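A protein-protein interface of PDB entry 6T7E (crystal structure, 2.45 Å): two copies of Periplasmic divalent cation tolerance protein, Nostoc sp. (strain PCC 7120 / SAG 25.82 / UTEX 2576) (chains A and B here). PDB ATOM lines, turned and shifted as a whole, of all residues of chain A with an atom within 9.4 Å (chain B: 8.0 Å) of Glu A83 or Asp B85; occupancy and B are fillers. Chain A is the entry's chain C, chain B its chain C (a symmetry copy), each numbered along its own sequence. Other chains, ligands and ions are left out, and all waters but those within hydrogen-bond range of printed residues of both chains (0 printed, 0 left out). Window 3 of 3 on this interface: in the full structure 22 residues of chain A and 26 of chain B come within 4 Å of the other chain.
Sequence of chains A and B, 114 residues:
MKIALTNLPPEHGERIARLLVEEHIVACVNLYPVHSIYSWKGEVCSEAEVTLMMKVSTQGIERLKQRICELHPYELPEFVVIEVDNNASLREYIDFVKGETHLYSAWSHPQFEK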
ATOM      1  N   MET A   1     -13.568   7.004  16.928  1.00  0.00           N
ATOM      2  CA  MET A   1     -14.234   7.878  15.925  1.00  0.00           C
ATOM      3  C   MET A   1     -15.496   8.512  16.491  1.00  0.00           C
ATOM      4  O   MET A   1     -15.976   8.132  17.561  1.00  0.00           O
ATOM      5  CB  MET A   1     -14.606   7.073  14.681  1.00  0.00           C
ATOM      6  CG  MET A   1     -15.628   5.979  14.949  1.00  0.00           C
ATOM      7  SD  MET A   1     -16.397   5.310  13.463  1.00  0.00           S
ATOM      8  CE  MET A   1     -17.164   6.762  12.746  1.00  0.00           C
ATOM      9  N   LYS A   2     -16.029   9.478  15.759  1.00  0.00           N
ATOM     10  CA  LYS A   2     -17.343  10.047  16.058  1.00  0.00           C
ATOM     11  C   LYS A   2     -18.067  10.251  14.732  1.00  0.00           C
ATOM     12  O   LYS A   2     -17.442  10.247  13.673  1.00  0.00           O
ATOM     13  CB  LYS A   2     -17.213  11.394  16.803  1.00  0.00           C
ATOM     14  CG  LYS A   2     -16.350  11.391  18.075  1.00  0.00           C
ATOM     15  CD  LYS A   2     -17.032  10.690  19.240  1.00  0.00           C
ATOM     16  CE  LYS A   2     -16.022  10.249  20.289  1.00  0.00           C
ATOM     17  N   ILE A   3     -19.385  10.406  14.781  1.00  0.00           N
ATOM     18  CA  ILE A   3     -20.113  10.912  13.632  1.00  0.00           C
ATOM     19  C   ILE A   3     -20.407  12.393  13.878  1.00  0.00           C
ATOM     20  O   ILE A   3     -20.753  12.775  14.988  1.00  0.00           O
ATOM     21  CB  ILE A   3     -21.401  10.116  13.358  1.00  0.00           C
ATOM     22  CG1 ILE A   3     -21.053   8.712  12.865  1.00  0.00           C
ATOM     23  CG2 ILE A   3     -22.247  10.806  12.304  1.00  0.00           C
ATOM     24  CD1 ILE A   3     -22.218   7.747  12.859  1.00  0.00           C
ATOM     25  N   ALA A   4     -20.222  13.219  12.853  1.00  0.00           N
ATOM     26  CA  ALA A   4     -20.628  14.612  12.889  1.00  0.00           C
ATOM     27  C   ALA A   4     -21.675  14.839  11.807  1.00  0.00           C
ATOM     28  O   ALA A   4     -21.593  14.250  10.719  1.00  0.00           O
ATOM     29  CB  ALA A   4     -19.436  15.524  12.663  1.00  0.00           C
ATOM     30  N   LEU A   5     -22.661  15.684  12.107  1.00  0.00           N
ATOM     31  CA  LEU A   5     -23.688  16.022  11.136  1.00  0.00           C
ATOM     32  C   LEU A   5     -23.687  17.495  10.818  1.00  0.00           C
ATOM     33  O   LEU A   5     -23.524  18.324  11.704  1.00  0.00           O
ATOM     34  CB  LEU A   5     -25.062  15.662  11.665  1.00  0.00           C
ATOM     35  CG  LEU A   5     -25.322  14.186  11.921  1.00  0.00           C
ATOM     36  CD1 LEU A   5     -26.709  14.063  12.545  1.00  0.00           C
ATOM     37  CD2 LEU A   5     -25.203  13.350  10.645  1.00  0.00           C
ATOM     38  N   THR A  58     -11.728  10.731  16.573  1.00  0.00           N
ATOM     39  CA  THR A  58     -12.019  11.548  17.750  1.00  0.00           C
ATOM     40  C   THR A  58     -11.149  12.792  17.795  1.00  0.00           C
ATOM     41  O   THR A  58     -11.656  13.890  17.979  1.00  0.00           O
ATOM     42  CB  THR A  58     -11.818  10.738  19.045  1.00  0.00           C
ATOM     43  OG1 THR A  58     -12.553   9.510  18.949  1.00  0.00           O
ATOM     44  CG2 THR A  58     -12.282  11.533  20.278  1.00  0.00           C
ATOM     45  N   ILE A  61     -11.890  15.882  15.315  1.00  0.00           N
ATOM     46  CA  ILE A  61     -13.184  16.569  15.379  1.00  0.00           C
ATOM     47  C   ILE A  61     -13.081  18.090  15.326  1.00  0.00           C
ATOM     48  O   ILE A  61     -13.865  18.738  14.628  1.00  0.00           O
ATOM     49  CB  ILE A  61     -13.975  16.146  16.637  1.00  0.00           C
ATOM     50  CG1 ILE A  61     -14.712  14.834  16.378  1.00  0.00           C
ATOM     51  CG2 ILE A  61     -14.985  17.211  17.055  1.00  0.00           C
ATOM     52  CD1 ILE A  61     -15.977  14.991  15.564  1.00  0.00           C
ATOM     53  N   LYS A  65     -14.704  20.628  12.784  1.00  0.00           N
ATOM     54  CA  LYS A  65     -15.522  21.758  13.199  1.00  0.00           C
ATOM     55  C   LYS A  65     -14.972  23.071  12.629  1.00  0.00           C
ATOM     56  O   LYS A  65     -15.723  23.879  12.064  1.00  0.00           O
ATOM     57  CB  LYS A  65     -15.599  21.844  14.722  1.00  0.00           C
ATOM     58  CG  LYS A  65     -16.502  22.966  15.201  1.00  0.00           C
ATOM     59  CD  LYS A  65     -17.158  22.672  16.540  1.00  0.00           C
ATOM     60  CE  LYS A  65     -16.261  23.016  17.704  1.00  0.00           C
ATOM     61  NZ  LYS A  65     -17.075  23.088  18.944  1.00  0.00           N
ATOM     62  N   PHE A  79     -23.473  22.091  13.243  1.00  0.00           N
ATOM     63  CA  PHE A  79     -22.439  21.099  13.454  1.00  0.00           C
ATOM     64  C   PHE A  79     -22.790  20.322  14.701  1.00  0.00           C
ATOM     65  O   PHE A  79     -22.735  20.848  15.798  1.00  0.00           O
ATOM     66  CB  PHE A  79     -21.050  21.722  13.571  1.00  0.00           C
ATOM     67  CG  PHE A  79     -19.953  20.701  13.595  1.00  0.00           C
ATOM     68  CD1 PHE A  79     -19.612  20.009  12.441  1.00  0.00           C
ATOM     69  CD2 PHE A  79     -19.292  20.397  14.771  1.00  0.00           C
ATOM     70  CE1 PHE A  79     -18.619  19.047  12.455  1.00  0.00           C
ATOM     71  CE2 PHE A  79     -18.286  19.438  14.795  1.00  0.00           C
ATOM     72  CZ  PHE A  79     -17.956  18.761  13.634  1.00  0.00           C
ATOM     73  N   VAL A  80     -23.181  19.071  14.517  1.00  0.00           N
ATOM     74  CA  VAL A  80     -23.658  18.265  15.616  1.00  0.00           C
ATOM     75  C   VAL A  80     -22.872  16.983  15.661  1.00  0.00           C
ATOM     76  O   VAL A  80     -22.822  16.259  14.672  1.00  0.00           O
ATOM     77  CB  VAL A  80     -25.141  17.923  15.441  1.00  0.00           C
ATOM     78  CG1 VAL A  80     -25.608  16.978  16.550  1.00  0.00           C
ATOM     79  CG2 VAL A  80     -25.959  19.200  15.436  1.00  0.00           C
ATOM     80  N   VAL A  81     -22.261  16.707  16.806  1.00  0.00           N
ATOM     81  CA  VAL A  81     -21.497  15.496  16.980  1.00  0.00           C
ATOM     82  C   VAL A  81     -22.315  14.452  17.729  1.00  0.00           C
ATOM     83  O   VAL A  81     -22.827  14.683  18.825  1.00  0.00           O
ATOM     84  CB  VAL A  81     -20.170  15.767  17.709  1.00  0.00           C
ATOM     85  CG1 VAL A  81     -19.411  14.466  17.952  1.00  0.00           C
ATOM     86  CG2 VAL A  81     -19.331  16.745  16.897  1.00  0.00           C
ATOM     87  N   ILE A  82     -22.394  13.288  17.108  1.00  0.00           N
ATOM     88  CA  ILE A  82     -23.140  12.148  17.607  1.00  0.00           C
ATOM     89  C   ILE A  82     -22.161  11.187  18.297  1.00  0.00           C
ATOM     90  O   ILE A  82     -21.030  11.003  17.830  1.00  0.00           O
ATOM     91  CB  ILE A  82     -23.913  11.516  16.422  1.00  0.00           C
ATOM     92  CG1 ILE A  82     -25.269  12.204  16.283  1.00  0.00           C
ATOM     93  CG2 ILE A  82     -24.119  10.024  16.584  1.00  0.00           C
ATOM     94  CD1 ILE A  82     -25.936  11.987  14.938  1.00  0.00           C
ATOM     95  N   GLU A  83     -22.583  10.601  19.416  1.00  0.00           N
ATOM     96  CA  GLU A  83     -21.704   9.757  20.238  1.00  0.00           C
ATOM     97  C   GLU A  83     -21.623   8.337  19.704  1.00  0.00           C
ATOM     98  O   GLU A  83     -22.617   7.616  19.700  1.00  0.00           O
ATOM     99  CB  GLU A  83     -22.230   9.677  21.668  1.00  0.00           C
ATOM    100  CG  GLU A  83     -22.345  11.007  22.397  1.00  0.00           C
ATOM    101  CD  GLU A  83     -21.127  11.338  23.224  1.00  0.00           C
ATOM    102  OE1 GLU A  83     -20.063  10.718  22.995  1.00  0.00           O
ATOM    103  OE2 GLU A  83     -21.240  12.226  24.099  1.00  0.00           O
ATOM    104  N   VAL A  84     -20.442   7.913  19.275  1.00  0.00           N
ATOM    105  CA  VAL A  84     -20.260   6.541  18.811  1.00  0.00           C
ATOM    106  C   VAL A  84     -19.806   5.651  19.965  1.00  0.00           C
ATOM    107  O   VAL A  84     -18.939   6.047  20.740  1.00  0.00           O
ATOM    108  CB  VAL A  84     -19.237   6.483  17.662  1.00  0.00           C
ATOM    109  CG1 VAL A  84     -18.854   5.042  17.340  1.00  0.00           C
ATOM    110  CG2 VAL A  84     -19.796   7.184  16.432  1.00  0.00           C
ATOM    111  N   ASP A  85     -20.397   4.460  20.077  1.00  0.00           N
ATOM    112  CA  ASP A  85     -19.911   3.427  21.004  1.00  0.00           C
ATOM    113  C   ASP A  85     -18.739   2.703  20.341  1.00  0.00           C
ATOM    114  O   ASP A  85     -18.926   1.771  19.553  1.00  0.00           O
ATOM    115  CB  ASP A  85     -21.028   2.434  21.367  1.00  0.00           C
ATOM    116  CG  ASP A  85     -20.612   1.425  22.436  1.00  0.00           C
ATOM    117  OD1 ASP A  85     -19.413   1.102  22.561  1.00  0.00           O
ATOM    118  OD2 ASP A  85     -21.495   0.933  23.157  1.00  0.00           O
ATOM    119  N   ASN A  86     -17.530   3.130  20.673  1.00  0.00           N
ATOM    120  CA  ASN A  86     -16.339   2.644  19.985  1.00  0.00           C
ATOM    121  C   ASN A  86     -16.021   1.173  20.241  1.00  0.00           C
ATOM    122  O   ASN A  86     -15.577   0.481  19.339  1.00  0.00           O
ATOM    123  CB  ASN A  86     -15.154   3.560  20.295  1.00  0.00           C
ATOM    124  CG  ASN A  86     -15.293   4.917  19.615  1.00  0.00           C
ATOM    125  OD1 ASN A  86     -15.008   5.054  18.430  1.00  0.00           O
ATOM    126  ND2 ASN A  86     -15.761   5.918  20.354  1.00  0.00           N
ATOM    127  N   SER A  89     -18.782  -0.895  18.138  1.00  0.00           N
ATOM    128  CA  SER A  89     -18.486  -0.792  16.707  1.00  0.00           C
ATOM    129  C   SER A  89     -17.330  -1.728  16.294  1.00  0.00           C
ATOM    130  O   SER A  89     -16.623  -2.274  17.137  1.00  0.00           O
ATOM    131  CB  SER A  89     -18.127   0.652  16.341  1.00  0.00           C
ATOM    132  OG  SER A  89     -19.091   1.568  16.829  1.00  0.00           O
ATOM    133  N   MET B   1     -28.421  20.085  23.786  1.00  0.00           N
ATOM    134  CA  MET B   1     -29.451  19.535  22.863  1.00  0.00           C
ATOM    135  C   MET B   1     -29.345  18.021  22.751  1.00  0.00           C
ATOM    136  O   MET B   1     -28.371  17.415  23.202  1.00  0.00           O
ATOM    137  CB  MET B   1     -29.297  20.141  21.470  1.00  0.00           C
ATOM    138  CG  MET B   1     -27.977  19.790  20.798  1.00  0.00           C
ATOM    139  SD  MET B   1     -27.943  20.119  19.027  1.00  0.00           S
ATOM    140  CE  MET B   1     -29.281  19.091  18.423  1.00  0.00           C
ATOM    141  N   LYS B   2     -30.355  17.421  22.139  1.00  0.00           N
ATOM    142  CA  LYS B   2     -30.311  16.005  21.772  1.00  0.00           C
ATOM    143  C   LYS B   2     -30.932  15.872  20.385  1.00  0.00           C
ATOM    144  O   LYS B   2     -31.623  16.777  19.922  1.00  0.00           O
ATOM    145  CB  LYS B   2     -31.092  15.140  22.786  1.00  0.00           C
ATOM    146  CG  LYS B   2     -30.703  15.303  24.264  1.00  0.00           C
ATOM    147  CD  LYS B   2     -29.362  14.662  24.588  1.00  0.00           C
ATOM    148  CE  LYS B   2     -28.763  15.243  25.859  1.00  0.00           C
ATOM    149  N   ILE B  82     -31.065  10.081  20.568  1.00  0.00           N
ATOM    150  CA  ILE B  82     -29.672   9.873  20.220  1.00  0.00           C
ATOM    151  C   ILE B  82     -28.812  10.832  21.055  1.00  0.00           C
ATOM    152  O   ILE B  82     -29.203  11.981  21.292  1.00  0.00           O
ATOM    153  CB  ILE B  82     -29.519  10.061  18.690  1.00  0.00           C
ATOM    154  CG1 ILE B  82     -29.778   8.729  17.992  1.00  0.00           C
ATOM    155  CG2 ILE B  82     -28.151  10.579  18.296  1.00  0.00           C
ATOM    156  CD1 ILE B  82     -30.076   8.857  16.509  1.00  0.00           C
ATOM    157  N   GLU B  83     -27.660  10.354  21.524  1.00  0.00           N
ATOM    158  CA  GLU B  83     -26.803  11.123  22.436  1.00  0.00           C
ATOM    159  C   GLU B  83     -25.917  12.104  21.685  1.00  0.00           C
ATOM    160  O   GLU B  83     -25.049  11.697  20.919  1.00  0.00           O
ATOM    161  CB  GLU B  83     -25.888  10.189  23.221  1.00  0.00           C
ATOM    162  CG  GLU B  83     -26.594   9.150  24.077  1.00  0.00           C
ATOM    163  CD  GLU B  83     -26.800   9.598  25.505  1.00  0.00           C
ATOM    164  OE1 GLU B  83     -26.695  10.818  25.769  1.00  0.00           O
ATOM    165  OE2 GLU B  83     -27.070   8.722  26.357  1.00  0.00           O
ATOM    166  N   VAL B  84     -26.107  13.396  21.915  1.00  0.00           N
ATOM    167  CA  VAL B  84     -25.253  14.403  21.290  1.00  0.00           C
ATOM    168  C   VAL B  84     -24.078  14.737  22.204  1.00  0.00           C
ATOM    169  O   VAL B  84     -24.265  14.901  23.407  1.00  0.00           O
ATOM    170  CB  VAL B  84     -26.055  15.678  20.970  1.00  0.00           C
ATOM    171  CG1 VAL B  84     -25.132  16.818  20.551  1.00  0.00           C
ATOM    172  CG2 VAL B  84     -27.084  15.386  19.887  1.00  0.00           C
ATOM    173  N   ASP B  85     -22.875  14.828  21.631  1.00  0.00           N
ATOM    174  CA  ASP B  85     -21.702  15.348  22.350  1.00  0.00           C
ATOM    175  C   ASP B  85     -21.757  16.875  22.312  1.00  0.00           C
ATOM    176  O   ASP B  85     -21.324  17.507  21.344  1.00  0.00           O
ATOM    177  CB  ASP B  85     -20.395  14.834  21.724  1.00  0.00           C
ATOM    178  CG  ASP B  85     -19.151  15.233  22.519  1.00  0.00           C
ATOM    179  OD1 ASP B  85     -19.157  16.269  23.215  1.00  0.00           O
ATOM    180  OD2 ASP B  85     -18.145  14.510  22.439  1.00  0.00           O
ATOM    181  N   ASN B  86     -22.282  17.464  23.377  1.00  0.00           N
ATOM    182  CA  ASN B  86     -22.550  18.898  23.393  1.00  0.00           C
ATOM    183  C   ASN B  86     -21.299  19.771  23.378  1.00  0.00           C
ATOM    184  O   ASN B  86     -21.295  20.817  22.746  1.00  0.00           O
ATOM    185  CB  ASN B  86     -23.482  19.235  24.559  1.00  0.00           C
ATOM    186  CG  ASN B  86     -24.898  18.722  24.318  1.00  0.00           C
ATOM    187  OD1 ASN B  86     -25.674  19.345  23.600  1.00  0.00           O
ATOM    188  ND2 ASN B  86     -25.230  17.570  24.893  1.00  0.00           N
ATOM    189  N   ASN B  87     -20.230  19.340  24.035  1.00  0.00           N
ATOM    190  CA  ASN B  87     -18.978  20.094  24.010  1.00  0.00           C
ATOM    191  C   ASN B  87     -18.295  20.097  22.632  1.00  0.00           C
ATOM    192  O   ASN B  87     -17.733  21.103  22.224  1.00  0.00           O
ATOM    193  CB  ASN B  87     -18.015  19.573  25.084  1.00  0.00           C
ATOM    194  CG  ASN B  87     -18.475  19.903  26.505  1.00  0.00           C
ATOM    195  OD1 ASN B  87     -19.299  20.800  26.719  1.00  0.00           O
ATOM    196  ND2 ASN B  87     -17.932  19.186  27.486  1.00  0.00           N
ATOM    197  N   ALA B  88     -18.352  18.981  21.917  1.00  0.00           N
ATOM    198  CA  ALA B  88     -17.714  18.870  20.602  1.00  0.00           C
ATOM    199  C   ALA B  88     -18.538  19.527  19.485  1.00  0.00           C
ATOM    200  O   ALA B  88     -17.978  20.027  18.511  1.00  0.00           O
ATOM    201  CB  ALA B  88     -17.448  17.409  20.272  1.00  0.00           C
ATOM    202  N   SER B  89     -19.861  19.505  19.612  1.00  0.00           N
ATOM    203  CA  SER B  89     -20.732  20.251  18.700  1.00  0.00           C
ATOM    204  C   SER B  89     -20.484  21.771  18.790  1.00  0.00           C
ATOM    205  O   SER B  89     -19.815  22.253  19.700  1.00  0.00           O
ATOM    206  CB  SER B  89     -22.204  19.955  19.011  1.00  0.00           C
ATOM    207  OG  SER B  89     -22.452  18.562  19.085  1.00  0.00           O
ATOM    208  N   LEU B  90     -21.033  22.516  17.834  1.00  0.00           N
ATOM    209  CA  LEU B  90     -20.862  23.966  17.795  1.00  0.00           C
ATOM    210  C   LEU B  90     -21.776  24.664  18.802  1.00  0.00           C
ATOM    211  O   LEU B  90     -23.000  24.509  18.767  1.00  0.00           O
ATOM    212  CB  LEU B  90     -21.136  24.502  16.387  1.00  0.00           C
ATOM    213  CG  LEU B  90     -20.822  25.997  16.194  1.00  0.00           C
ATOM    214  CD1 LEU B  90     -19.328  26.270  16.341  1.00  0.00           C
ATOM    215  CD2 LEU B  90     -21.341  26.493  14.842  1.00  0.00           C
ATOM    216  N   ILE B  94     -26.073  24.830  19.246  1.00  0.00           N
ATOM    217  CA  ILE B  94     -26.774  24.322  20.433  1.00  0.00           C
ATOM    218  C   ILE B  94     -27.623  25.426  21.054  1.00  0.00           C
ATOM    219  O   ILE B  94     -28.775  25.200  21.422  1.00  0.00           O
ATOM    220  CB  ILE B  94     -25.790  23.788  21.495  1.00  0.00           C
ATOM    221  CG1 ILE B  94     -25.103  22.524  20.981  1.00  0.00           C
ATOM    222  CG2 ILE B  94     -26.497  23.503  22.819  1.00  0.00           C
ATOM    223  CD1 ILE B  94     -24.003  22.030  21.894  1.00  0.00           C
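The backbone NH (N) of Glu A83 sits at hydrogen-bond distance from the backbone carbonyl oxygen (O) of Glu B83 (3.1 Å).
The side-chain amino group (NZ) of Lys A65 is in hydrogen-bond range of the backbone carbonyl oxygen (O) of Ala B88, at 3.2 Å.
O of Val A81 lies within hydrogen-bond range of N of Asp B85 (2.8 Å).
NZ of Lys A65 sits at hydrogen-bond distance from O of Ser B89 (3.0 Å).
O of Phe A79 is in hydrogen-bond range of N of Leu B90, at 3.1 Å.
The side-chain hydroxyl (OG) of Ser B89 is in hydrogen-bond range of the backbone NH (N) of Val A81 (2.9 Å).
The backbone NH of Ala B88 lies within hydrogen-bond range of the side-chain carboxylate of Asp B85 (3.1 Å).
The backbone NH (N) of Asn B87 sits at hydrogen-bond distance from the side-chain carboxylate (OD1) of Asp B85 (3.4 Å).
The backbone carbonyl oxygen (O) of Asp B85 is in hydrogen-bond range of the side-chain hydroxyl (OG) of Ser B89 (2.7 Å).
The backbone NH (N) of Leu A5 sits at hydrogen-bond distance from the backbone carbonyl oxygen (O) of Val A80.
O of Val B84 lies within hydrogen-bond range of ND2 of Asn B86 (3.2 Å).
O of Ile A3 is in hydrogen-bond range of N of Ile A82.
Among the printed residues, merely in contact across the chains: Phe A79 with Ser B89, Val A81 with Val B84, Glu A83 with Asp B85, Val A80 with Ser B89, Phe A79 with Ala B88, Ile A82 with Glu B83, Ile A82 with Ile B82, Val A81 with Ala B88, Lys A65 with Asn B87 and Val A80 with Val B84.
Glu A83 touches just these residues of chain B: Glu B83 (3.1 Å) and Asp B85 (3.6 Å).
Asp B85 touches just these residues of chain A: Val A81 and Glu A83.
No residue of chain A comes within 4 Å of Asn B86.
Ala B88 touches three residues of chain A.
Ser B89 touches just these residues of chain A: Lys A65, Phe A79, Val A80 and Val A81.
Of the printed residues of chain B, Val A81 touches Val B84 (3.5 Å), Asp B85 (2.8 Å), Ala B88 (3.9 Å) and Ser B89 (2.9 Å).
Printed residues of chain A within 4 Å of Leu B90: Phe A79.
Of the printed residues of chain A, Glu B83 touches Ile A82 and Glu A83.
Of the printed residues of chain A, Ile B82 touches Ile A82 (3.9 Å).
Of the printed residues of chain B, Phe A79 touches Ala B88 (3.8 Å), Ser B89 (3.4 Å) and Leu B90 (3.1 Å).
Asp A85 touches none of the printed residues of chain B.
The nearest residue of chain B that does not touch Glu A83 is Val B84 (4.1 Å).
Hydrophobic or aromatic side chains of chain B that line the printed part of chain A: Ile B82, Val B84, Ala B88 and Leu B90.
Along chain B the printed residues that touch a printed residue of chain A span positions 82 to 90.
Hydrophobic or aromatic side chains of chain A within 4 Å of the printed part of chain B: Phe A79, Val A80, Val A81 and Ile A82.
Among the printed residues, no Asp or Glu carboxylate lies within 4 Å of a Lys or Arg side-chain nitrogen of the other chain.
Ile B82 touches its own counterpart, Ile A82.
Ile A82 touches Glu B83, but with the chains exchanged Glu A83 does not touch Ile B82 (5.7 Å).
Glu A83 touches its own counterpart, Glu B83.
Glu A83 touches Asp B85, but with the chains exchanged Asp A85 does not touch Glu B83 (8.5 Å).
8 positions are printed for both chains.
Of the 16 pairs that touch across the chains among the printed residues, 2 have their exchanged pair printed and touching as well.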
